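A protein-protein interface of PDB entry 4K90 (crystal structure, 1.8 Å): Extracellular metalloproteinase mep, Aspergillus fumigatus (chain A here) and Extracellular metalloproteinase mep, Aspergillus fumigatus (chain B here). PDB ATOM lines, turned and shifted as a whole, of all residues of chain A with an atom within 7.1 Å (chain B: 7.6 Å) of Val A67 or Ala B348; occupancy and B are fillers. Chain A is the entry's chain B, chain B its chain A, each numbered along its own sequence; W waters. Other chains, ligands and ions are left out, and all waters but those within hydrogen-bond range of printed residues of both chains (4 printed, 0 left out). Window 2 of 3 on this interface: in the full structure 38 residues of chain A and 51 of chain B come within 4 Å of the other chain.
The side-chain amide nitrogen of Asn A89 is in hydrogen-bond range of the backbone carbonyl oxygen of Leu B328, at 3.0 Å.
The backbone carbonyl oxygen of Ala B327 sits at hydrogen-bond distance from a ring nitrogen (ND1) of His A69, 3.3 Å away.
The backbone carbonyl oxygen of Leu B343 lies within hydrogen-bond range of the side-chain hydroxyl of Thr B347, 3.3 Å away.
The side-chain amide oxygen (OD1) of Asn A89 is in hydrogen-bond range of a ring nitrogen (ND1) of His A69 (2.9 Å).
N of Asn A89 is in hydrogen-bond range of O of Ser A98, at 2.9 Å.
The backbone NH (N) of Val A67 sits at hydrogen-bond distance from the side-chain amide oxygen (OD1) of Asn A65, at 3.2 Å.
O of Val A67 sits at hydrogen-bond distance from NE2 of His A69, at 3.4 Å.
The backbone NH (N) of Phe A97 lies within hydrogen-bond range of the backbone carbonyl oxygen (O) of Asn A89 (2.7 Å).
OH of Tyr A61 touches CB of Ala B327, at 3.7 Å.
Asp B324 touches Asn A65.
Ala B348 touches Val A67 (CB to CG2, 3.8 Å).
CD2 of Leu B328 touches CE1 of His A69, 3.8 Å away.
Asn A89 touches Ala B327.
Phe A97 touches Asp B344 (CZ to O, 3.3 Å).
CG2 of Thr B347 touches CE1 of Phe A97, at 3.98 Å.
Ala B348 touches Phe A97 (CB to CZ, 3.9 Å).
Gly A66 touches none of the printed residues of chain B.
Of chain B, only Ala B348 (3.8 Å) comes within 4 Å of Val A67.
Ala A68 touches none of the printed residues of chain B.
Of the printed residues of chain B, Asn A89 touches Ala B327 (3.6 Å) and Leu B328 (3.0 Å).
Val B310 touches none of the printed residues of chain A.
Of the printed residues of chain A, Leu B328 touches His A69 and Asn A89.
Printed residues of chain A within 4 Å of Asp B344: Phe A97.
The nearest residue of chain B that does not touch Val A67 is Leu B328 (4.1 Å).
Along chain A the printed residues that touch a printed residue of chain B span positions 61 to 97.
Along chain B the printed residues that touch a printed residue of chain A span positions 324 to 348.
Among the printed residues, 10 pairs touch across the chains.
Among the printed residues, no Asp or Glu carboxylate lies within 4 Å of a Lys or Arg side-chain nitrogen of the other chain.
Water W4 bridges OD1 of Asn A89 (2.7 Å) and O of Ala B327 (2.9 Å).
Water W2 lies within hydrogen-bond range of the backbone carbonyl oxygen (O) of Ala B345, the side-chain amide nitrogen (ND2) of Asn A65 and the side-chain carboxylate (OD2) of Asp B324.
Water W3 bridges the backbone carbonyl oxygen (O) of Ala B348 and the backbone carbonyl oxygen (O) of Asn A65.
Water W1 lies within hydrogen-bond range of O of Asp B324 (2.9 Å), ND2 of Asn A65 (3.2 Å) and NE2 of His A69 (3.5 Å).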
ATOM      1  N   TYR A  37     -12.768  29.325  14.202  1.00  0.00           N
ATOM      2  CA  TYR A  37     -12.152  28.025  14.535  1.00  0.00           C
ATOM      3  C   TYR A  37     -13.202  26.954  14.827  1.00  0.00           C
ATOM      4  O   TYR A  37     -12.994  25.770  14.541  1.00  0.00           O
ATOM      5  CB  TYR A  37     -11.138  28.150  15.682  1.00  0.00           C
ATOM      6  CG  TYR A  37     -11.709  28.450  17.053  1.00  0.00           C
ATOM      7  CD1 TYR A  37     -12.209  27.422  17.857  1.00  0.00           C
ATOM      8  CD2 TYR A  37     -11.676  29.743  17.590  1.00  0.00           C
ATOM      9  CE1 TYR A  37     -12.695  27.669  19.130  1.00  0.00           C
ATOM     10  CE2 TYR A  37     -12.180  30.008  18.867  1.00  0.00           C
ATOM     11  CZ  TYR A  37     -12.680  28.962  19.636  1.00  0.00           C
ATOM     12  OH  TYR A  37     -13.175  29.167  20.910  1.00  0.00           O
ATOM     13  N   TYR A  61     -11.943  27.101  23.487  1.00  0.00           N
ATOM     14  CA  TYR A  61     -11.186  28.323  23.757  1.00  0.00           C
ATOM     15  C   TYR A  61      -9.939  28.373  22.919  1.00  0.00           C
ATOM     16  O   TYR A  61      -9.508  27.344  22.374  1.00  0.00           O
ATOM     17  CB  TYR A  61     -10.837  28.431  25.256  1.00  0.00           C
ATOM     18  CG  TYR A  61      -9.879  27.371  25.751  1.00  0.00           C
ATOM     19  CD1 TYR A  61      -8.509  27.656  25.897  1.00  0.00           C
ATOM     20  CD2 TYR A  61     -10.324  26.072  26.058  1.00  0.00           C
ATOM     21  CE1 TYR A  61      -7.615  26.693  26.357  1.00  0.00           C
ATOM     22  CE2 TYR A  61      -9.406  25.088  26.518  1.00  0.00           C
ATOM     23  CZ  TYR A  61      -8.069  25.414  26.656  1.00  0.00           C
ATOM     24  OH  TYR A  61      -7.150  24.482  27.113  1.00  0.00           O
ATOM     25  N   VAL A  62      -9.366  29.571  22.816  1.00  0.00           N
ATOM     26  CA  VAL A  62      -8.069  29.763  22.171  1.00  0.00           C
ATOM     27  C   VAL A  62      -6.998  29.851  23.265  1.00  0.00           C
ATOM     28  O   VAL A  62      -7.060  30.714  24.154  1.00  0.00           O
ATOM     29  CB  VAL A  62      -8.015  31.033  21.296  1.00  0.00           C
ATOM     30  CG1 VAL A  62      -6.701  31.106  20.518  1.00  0.00           C
ATOM     31  CG2 VAL A  62      -9.188  31.091  20.351  1.00  0.00           C
ATOM     32  N   GLY A  63      -6.026  28.949  23.190  1.00  0.00           N
ATOM     33  CA  GLY A  63      -4.935  28.907  24.165  1.00  0.00           C
ATOM     34  C   GLY A  63      -3.979  30.067  23.983  1.00  0.00           C
ATOM     35  O   GLY A  63      -3.923  30.677  22.911  1.00  0.00           O
ATOM     36  N   ASP A  64      -3.216  30.387  25.030  1.00  0.00           N
ATOM     37  CA  ASP A  64      -2.242  31.475  24.904  1.00  0.00           C
ATOM     38  C   ASP A  64      -1.099  31.136  23.949  1.00  0.00           C
ATOM     39  O   ASP A  64      -0.250  31.986  23.663  1.00  0.00           O
ATOM     40  CB  ASP A  64      -1.752  31.996  26.273  1.00  0.00           C
ATOM     41  CG  ASP A  64      -0.927  30.978  27.053  1.00  0.00           C
ATOM     42  OD1 ASP A  64      -0.641  29.888  26.537  1.00  0.00           O
ATOM     43  OD2 ASP A  64      -0.561  31.286  28.207  1.00  0.00           O
ATOM     44  N   ASN A  65      -1.076  29.901  23.439  1.00  0.00           N
ATOM     45  CA  ASN A  65      -0.192  29.576  22.308  1.00  0.00           C
ATOM     46  C   ASN A  65      -0.776  29.925  20.919  1.00  0.00           C
ATOM     47  O   ASN A  65      -0.084  29.824  19.911  1.00  0.00           O
ATOM     48  CB  ASN A  65       0.296  28.113  22.372  1.00  0.00           C
ATOM     49  CG  ASN A  65      -0.846  27.093  22.392  1.00  0.00           C
ATOM     50  OD1 ASN A  65      -2.034  27.451  22.398  1.00  0.00           O
ATOM     51  ND2 ASN A  65      -0.485  25.812  22.412  1.00  0.00           N
ATOM     52  N   GLY A  66      -2.044  30.342  20.862  1.00  0.00           N
ATOM     53  CA  GLY A  66      -2.688  30.658  19.587  1.00  0.00           C
ATOM     54  C   GLY A  66      -3.455  29.477  18.982  1.00  0.00           C
ATOM     55  O   GLY A  66      -4.155  29.618  17.991  1.00  0.00           O
ATOM     56  N   VAL A  67      -3.334  28.309  19.592  1.00  0.00           N
ATOM     57  CA  VAL A  67      -4.074  27.138  19.130  1.00  0.00           C
ATOM     58  C   VAL A  67      -5.439  27.091  19.818  1.00  0.00           C
ATOM     59  O   VAL A  67      -5.531  27.197  21.053  1.00  0.00           O
ATOM     60  CB  VAL A  67      -3.280  25.824  19.409  1.00  0.00           C
ATOM     61  CG1 VAL A  67      -4.041  24.616  18.904  1.00  0.00           C
ATOM     62  CG2 VAL A  67      -1.895  25.894  18.760  1.00  0.00           C
ATOM     63  N   ALA A  68      -6.497  26.924  19.025  1.00  0.00           N
ATOM     64  CA  ALA A  68      -7.847  26.778  19.562  1.00  0.00           C
ATOM     65  C   ALA A  68      -8.162  25.300  19.784  1.00  0.00           C
ATOM     66  O   ALA A  68      -7.681  24.441  19.044  1.00  0.00           O
ATOM     67  CB  ALA A  68      -8.867  27.395  18.627  1.00  0.00           C
ATOM     68  N   HIS A  69      -8.949  25.012  20.812  1.00  0.00           N
ATOM     69  CA  HIS A  69      -9.325  23.635  21.134  1.00  0.00           C
ATOM     70  C   HIS A  69     -10.827  23.543  21.149  1.00  0.00           C
ATOM     71  O   HIS A  69     -11.488  24.302  21.875  1.00  0.00           O
ATOM     72  CB  HIS A  69      -8.774  23.239  22.512  1.00  0.00           C
ATOM     73  CG  HIS A  69      -7.339  23.612  22.703  1.00  0.00           C
ATOM     74  ND1 HIS A  69      -6.305  22.901  22.134  1.00  0.00           N
ATOM     75  CD2 HIS A  69      -6.769  24.641  23.374  1.00  0.00           C
ATOM     76  CE1 HIS A  69      -5.156  23.462  22.466  1.00  0.00           C
ATOM     77  NE2 HIS A  69      -5.409  24.524  23.213  1.00  0.00           N
ATOM     78  N   VAL A  88     -10.547  18.737  18.459  1.00  0.00           N
ATOM     79  CA  VAL A  88      -9.886  19.352  17.317  1.00  0.00           C
ATOM     80  C   VAL A  88      -9.070  20.555  17.762  1.00  0.00           C
ATOM     81  O   VAL A  88      -9.601  21.473  18.406  1.00  0.00           O
ATOM     82  CB  VAL A  88     -10.901  19.799  16.217  1.00  0.00           C
ATOM     83  CG1 VAL A  88     -10.136  20.366  15.017  1.00  0.00           C
ATOM     84  CG2 VAL A  88     -11.775  18.634  15.797  1.00  0.00           C
ATOM     85  N   ASN A  89      -7.784  20.525  17.425  1.00  0.00           N
ATOM     86  CA  ASN A  89      -6.880  21.638  17.654  1.00  0.00           C
ATOM     87  C   ASN A  89      -6.680  22.400  16.356  1.00  0.00           C
ATOM     88  O   ASN A  89      -6.233  21.834  15.358  1.00  0.00           O
ATOM     89  CB  ASN A  89      -5.538  21.131  18.192  1.00  0.00           C
ATOM     90  CG  ASN A  89      -5.709  20.233  19.402  1.00  0.00           C
ATOM     91  OD1 ASN A  89      -6.316  20.630  20.400  1.00  0.00           O
ATOM     92  ND2 ASN A  89      -5.218  18.982  19.301  1.00  0.00           N
ATOM     93  N   VAL A  90      -7.028  23.680  16.387  1.00  0.00           N
ATOM     94  CA  VAL A  90      -6.961  24.539  15.211  1.00  0.00           C
ATOM     95  C   VAL A  90      -5.786  25.501  15.372  1.00  0.00           C
ATOM     96  O   VAL A  90      -5.716  26.258  16.347  1.00  0.00           O
ATOM     97  CB  VAL A  90      -8.294  25.315  15.003  1.00  0.00           C
ATOM     98  CG1 VAL A  90      -8.260  26.115  13.700  1.00  0.00           C
ATOM     99  CG2 VAL A  90      -9.489  24.360  14.981  1.00  0.00           C
ATOM    100  N   GLY A  91      -4.856  25.450  14.423  1.00  0.00           N
ATOM    101  CA  GLY A  91      -3.663  26.312  14.450  1.00  0.00           C
ATOM    102  C   GLY A  91      -3.993  27.787  14.316  1.00  0.00           C
ATOM    103  O   GLY A  91      -5.094  28.149  13.887  1.00  0.00           O
ATOM    104  N   LYS A  92      -3.044  28.647  14.671  1.00  0.00           N
ATOM    105  CA  LYS A  92      -3.261  30.091  14.521  1.00  0.00           C
ATOM    106  C   LYS A  92      -3.455  30.477  13.045  1.00  0.00           C
ATOM    107  O   LYS A  92      -4.022  31.526  12.747  1.00  0.00           O
ATOM    108  CB  LYS A  92      -2.159  30.925  15.212  1.00  0.00           C
ATOM    109  CG  LYS A  92      -0.762  30.728  14.666  1.00  0.00           C
ATOM    110  CD  LYS A  92       0.274  31.540  15.449  1.00  0.00           C
ATOM    111  CE  LYS A  92       1.681  31.030  15.154  1.00  0.00           C
ATOM    112  NZ  LYS A  92       2.694  32.105  15.329  1.00  0.00           N
ATOM    113  N   PHE A  97      -4.755  21.687  13.157  1.00  0.00           N
ATOM    114  CA  PHE A  97      -3.354  21.422  13.516  1.00  0.00           C
ATOM    115  C   PHE A  97      -3.131  19.945  13.874  1.00  0.00           C
ATOM    116  O   PHE A  97      -2.155  19.315  13.405  1.00  0.00           O
ATOM    117  CB  PHE A  97      -2.932  22.357  14.663  1.00  0.00           C
ATOM    118  CG  PHE A  97      -1.564  22.075  15.239  1.00  0.00           C
ATOM    119  CD1 PHE A  97      -0.410  22.312  14.504  1.00  0.00           C
ATOM    120  CD2 PHE A  97      -1.441  21.617  16.556  1.00  0.00           C
ATOM    121  CE1 PHE A  97       0.861  22.059  15.063  1.00  0.00           C
ATOM    122  CE2 PHE A  97      -0.184  21.373  17.118  1.00  0.00           C
ATOM    123  CZ  PHE A  97       0.958  21.593  16.380  1.00  0.00           C
ATOM    124  N   SER A  98      -4.033  19.409  14.693  1.00  0.00           N
ATOM    125  CA  SER A  98      -4.021  17.989  15.092  1.00  0.00           C
ATOM    126  C   SER A  98      -5.381  17.686  15.692  1.00  0.00           C
ATOM    127  O   SER A  98      -6.143  18.608  15.992  1.00  0.00           O
ATOM    128  CB  SER A  98      -2.891  17.672  16.091  1.00  0.00           C
ATOM    129  OG  SER A  98      -3.124  18.270  17.359  1.00  0.00           O
ATOM    130  N   VAL B 310       6.780  32.503  25.150  1.00  0.00           N
ATOM    131  CA  VAL B 310       7.637  31.331  25.320  1.00  0.00           C
ATOM    132  C   VAL B 310       8.538  31.533  26.546  1.00  0.00           C
ATOM    133  O   VAL B 310       9.234  32.545  26.635  1.00  0.00           O
ATOM    134  CB  VAL B 310       8.508  31.073  24.070  1.00  0.00           C
ATOM    135  CG1 VAL B 310       9.301  29.785  24.218  1.00  0.00           C
ATOM    136  CG2 VAL B 310       7.644  31.037  22.787  1.00  0.00           C
ATOM    137  N   LEU B 321       5.349  23.121  28.003  1.00  0.00           N
ATOM    138  CA  LEU B 321       5.088  22.124  26.961  1.00  0.00           C
ATOM    139  C   LEU B 321       4.232  20.977  27.476  1.00  0.00           C
ATOM    140  O   LEU B 321       3.355  20.474  26.767  1.00  0.00           O
ATOM    141  CB  LEU B 321       6.386  21.606  26.345  1.00  0.00           C
ATOM    142  CG  LEU B 321       7.203  22.621  25.545  1.00  0.00           C
ATOM    143  CD1 LEU B 321       8.493  21.969  25.056  1.00  0.00           C
ATOM    144  CD2 LEU B 321       6.370  23.171  24.382  1.00  0.00           C
ATOM    145  N   ASP B 324       0.659  22.379  27.702  1.00  0.00           N
ATOM    146  CA  ASP B 324       0.105  22.552  26.355  1.00  0.00           C
ATOM    147  C   ASP B 324      -0.220  21.185  25.745  1.00  0.00           C
ATOM    148  O   ASP B 324      -1.240  21.028  25.059  1.00  0.00           O
ATOM    149  CB  ASP B 324       1.095  23.322  25.458  1.00  0.00           C
ATOM    150  CG  ASP B 324       1.137  24.823  25.774  1.00  0.00           C
ATOM    151  OD1 ASP B 324       0.339  25.289  26.611  1.00  0.00           O
ATOM    152  OD2 ASP B 324       1.981  25.529  25.183  1.00  0.00           O
ATOM    153  N   ALA B 327      -3.608  19.868  26.765  1.00  0.00           N
ATOM    154  CA  ALA B 327      -4.721  20.506  26.055  1.00  0.00           C
ATOM    155  C   ALA B 327      -4.886  20.011  24.599  1.00  0.00           C
ATOM    156  O   ALA B 327      -5.957  20.188  23.999  1.00  0.00           O
ATOM    157  CB  ALA B 327      -4.571  22.033  26.091  1.00  0.00           C
ATOM    158  N   LEU B 328      -3.844  19.402  24.043  1.00  0.00           N
ATOM    159  CA  LEU B 328      -3.874  18.893  22.655  1.00  0.00           C
ATOM    160  C   LEU B 328      -4.342  17.427  22.569  1.00  0.00           C
ATOM    161  O   LEU B 328      -4.999  17.025  21.597  1.00  0.00           O
ATOM    162  CB  LEU B 328      -2.488  19.009  21.997  1.00  0.00           C
ATOM    163  CG  LEU B 328      -1.858  20.386  21.722  1.00  0.00           C
ATOM    164  CD1 LEU B 328      -0.420  20.232  21.253  1.00  0.00           C
ATOM    165  CD2 LEU B 328      -2.692  21.158  20.652  1.00  0.00           C
ATOM    166  N   ALA B 341       1.690  14.593  21.592  1.00  0.00           N
ATOM    167  CA  ALA B 341       1.061  15.853  21.994  1.00  0.00           C
ATOM    168  C   ALA B 341       2.085  16.844  22.561  1.00  0.00           C
ATOM    169  O   ALA B 341       1.993  18.054  22.324  1.00  0.00           O
ATOM    170  CB  ALA B 341      -0.080  15.590  22.988  1.00  0.00           C
ATOM    171  N   ILE B 342       3.080  16.334  23.287  1.00  0.00           N
ATOM    172  CA  ILE B 342       4.140  17.191  23.806  1.00  0.00           C
ATOM    173  C   ILE B 342       5.007  17.719  22.666  1.00  0.00           C
ATOM    174  O   ILE B 342       5.334  18.906  22.632  1.00  0.00           O
ATOM    175  CB  ILE B 342       4.988  16.478  24.886  1.00  0.00           C
ATOM    176  CG1 ILE B 342       4.173  16.361  26.182  1.00  0.00           C
ATOM    177  CG2 ILE B 342       6.304  17.275  25.165  1.00  0.00           C
ATOM    178  CD1 ILE B 342       4.765  15.324  27.186  1.00  0.00           C
ATOM    179  N   LEU B 343       5.366  16.825  21.736  1.00  0.00           N
ATOM    180  CA  LEU B 343       6.117  17.221  20.547  1.00  0.00           C
ATOM    181  C   LEU B 343       5.363  18.264  19.704  1.00  0.00           C
ATOM    182  O   LEU B 343       5.965  19.256  19.238  1.00  0.00           O
ATOM    183  CB  LEU B 343       6.517  15.987  19.728  1.00  0.00           C
ATOM    184  CG  LEU B 343       7.662  15.162  20.367  1.00  0.00           C
ATOM    185  CD1 LEU B 343       7.628  13.692  19.970  1.00  0.00           C
ATOM    186  CD2 LEU B 343       9.041  15.784  20.065  1.00  0.00           C
ATOM    187  N   ASP B 344       4.051  18.078  19.573  1.00  0.00           N
ATOM    188  CA  ASP B 344       3.197  19.010  18.825  1.00  0.00           C
ATOM    189  C   ASP B 344       3.048  20.336  19.559  1.00  0.00           C
ATOM    190  O   ASP B 344       2.977  21.396  18.934  1.00  0.00           O
ATOM    191  CB  ASP B 344       1.818  18.394  18.556  1.00  0.00           C
ATOM    192  CG  ASP B 344       1.851  17.263  17.517  1.00  0.00           C
ATOM    193  OD1 ASP B 344       2.890  17.033  16.828  1.00  0.00           O
ATOM    194  OD2 ASP B 344       0.805  16.591  17.394  1.00  0.00           O
ATOM    195  N   ALA B 345       3.027  20.278  20.893  1.00  0.00           N
ATOM    196  CA  ALA B 345       3.074  21.496  21.706  1.00  0.00           C
ATOM    197  C   ALA B 345       4.315  22.336  21.391  1.00  0.00           C
ATOM    198  O   ALA B 345       4.219  23.554  21.262  1.00  0.00           O
ATOM    199  CB  ALA B 345       3.027  21.156  23.185  1.00  0.00           C
ATOM    200  N   ASP B 346       5.473  21.687  21.273  1.00  0.00           N
ATOM    201  CA  ASP B 346       6.698  22.416  20.935  1.00  0.00           C
ATOM    202  C   ASP B 346       6.637  22.991  19.507  1.00  0.00           C
ATOM    203  O   ASP B 346       7.059  24.131  19.274  1.00  0.00           O
ATOM    204  CB  ASP B 346       7.933  21.536  21.098  1.00  0.00           C
ATOM    205  CG  ASP B 346       9.207  22.284  20.747  1.00  0.00           C
ATOM    206  OD1 ASP B 346       9.477  23.311  21.409  1.00  0.00           O
ATOM    207  OD2 ASP B 346       9.897  21.853  19.802  1.00  0.00           O
ATOM    208  N   THR B 347       6.074  22.225  18.576  1.00  0.00           N
ATOM    209  CA  THR B 347       5.843  22.728  17.212  1.00  0.00           C
ATOM    210  C   THR B 347       4.988  23.995  17.240  1.00  0.00           C
ATOM    211  O   THR B 347       5.330  25.005  16.597  1.00  0.00           O
ATOM    212  CB  THR B 347       5.214  21.652  16.324  1.00  0.00           C
ATOM    213  OG1 THR B 347       6.157  20.581  16.176  1.00  0.00           O
ATOM    214  CG2 THR B 347       4.838  22.217  14.924  1.00  0.00           C
ATOM    215  N   ALA B 348       3.896  23.961  18.005  1.00  0.00           N
ATOM    216  CA  ALA B 348       2.987  25.107  18.106  1.00  0.00           C
ATOM    217  C   ALA B 348       3.568  26.301  18.862  1.00  0.00           C
ATOM    218  O   ALA B 348       3.229  27.459  18.564  1.00  0.00           O
ATOM    219  CB  ALA B 348       1.660  24.683  18.726  1.00  0.00           C
ATOM    220  N   LEU B 349       4.441  26.032  19.831  1.00  0.00           N
ATOM    221  CA  LEU B 349       4.929  27.105  20.700  1.00  0.00           C
ATOM    222  C   LEU B 349       6.194  27.768  20.168  1.00  0.00           C
ATOM    223  O   LEU B 349       6.302  29.002  20.182  1.00  0.00           O
ATOM    224  CB  LEU B 349       5.162  26.592  22.138  1.00  0.00           C
ATOM    225  CG  LEU B 349       5.543  27.680  23.158  1.00  0.00           C
ATOM    226  CD1 LEU B 349       4.351  28.581  23.469  1.00  0.00           C
ATOM    227  CD2 LEU B 349       6.103  27.062  24.427  1.00  0.00           C
ATOM    228  N   THR B 350       7.135  26.951  19.690  1.00  0.00           N
ATOM    229  CA  THR B 350       8.466  27.434  19.319  1.00  0.00           C
ATOM    230  C   THR B 350       8.772  27.244  17.825  1.00  0.00           C
ATOM    231  O   THR B 350       9.863  27.590  17.358  1.00  0.00           O
ATOM    232  CB  THR B 350       9.590  26.719  20.149  1.00  0.00           C
ATOM    233  OG1 THR B 350       9.791  25.385  19.656  1.00  0.00           O
ATOM    234  CG2 THR B 350       9.263  26.677  21.649  1.00  0.00           C
ATOM    235  N   GLY B 351       7.827  26.679  17.077  1.00  0.00           N
ATOM    236  CA  GLY B 351       8.095  26.268  15.697  1.00  0.00           C
ATOM    237  C   GLY B 351       8.917  24.994  15.627  1.00  0.00           C
ATOM    238  O   GLY B 351       9.487  24.669  14.582  1.00  0.00           O
ATOM    239  N   GLY B 352       8.980  24.258  16.738  1.00  0.00           N
ATOM    240  CA  GLY B 352       9.634  22.958  16.751  1.00  0.00           C
ATOM    241  C   GLY B 352      11.130  23.015  17.008  1.00  0.00           C
ATOM    242  O   GLY B 352      11.877  22.170  16.529  1.00  0.00           O
ATOM    243  N   GLN B 355      12.526  19.654  19.125  1.00  0.00           N
ATOM    244  CA  GLN B 355      12.129  18.305  18.741  1.00  0.00           C
ATOM    245  C   GLN B 355      13.224  17.293  19.089  1.00  0.00           C
ATOM    246  O   GLN B 355      12.933  16.224  19.618  1.00  0.00           O
ATOM    247  CB  GLN B 355      11.765  18.236  17.256  1.00  0.00           C
ATOM    248  CG  GLN B 355      10.599  19.139  16.850  1.00  0.00           C
ATOM    249  CD  GLN B 355       9.290  18.705  17.470  1.00  0.00           C
ATOM    250  OE1 GLN B 355       8.692  17.716  17.050  1.00  0.00           O
ATOM    251  NE2 GLN B 355       8.834  19.446  18.474  1.00  0.00           N
HETATM  252  O   HOH W   1      -2.176  23.384  23.620  1.00  0.00           O
HETATM  253  O   HOH W   2       2.087  24.746  22.502  1.00  0.00           O
HETATM  254  O   HOH W   3       0.855  28.374  17.542  1.00  0.00           O
HETATM  255  O   HOH W   4      -7.940  19.273  22.031  1.00  0.00           O
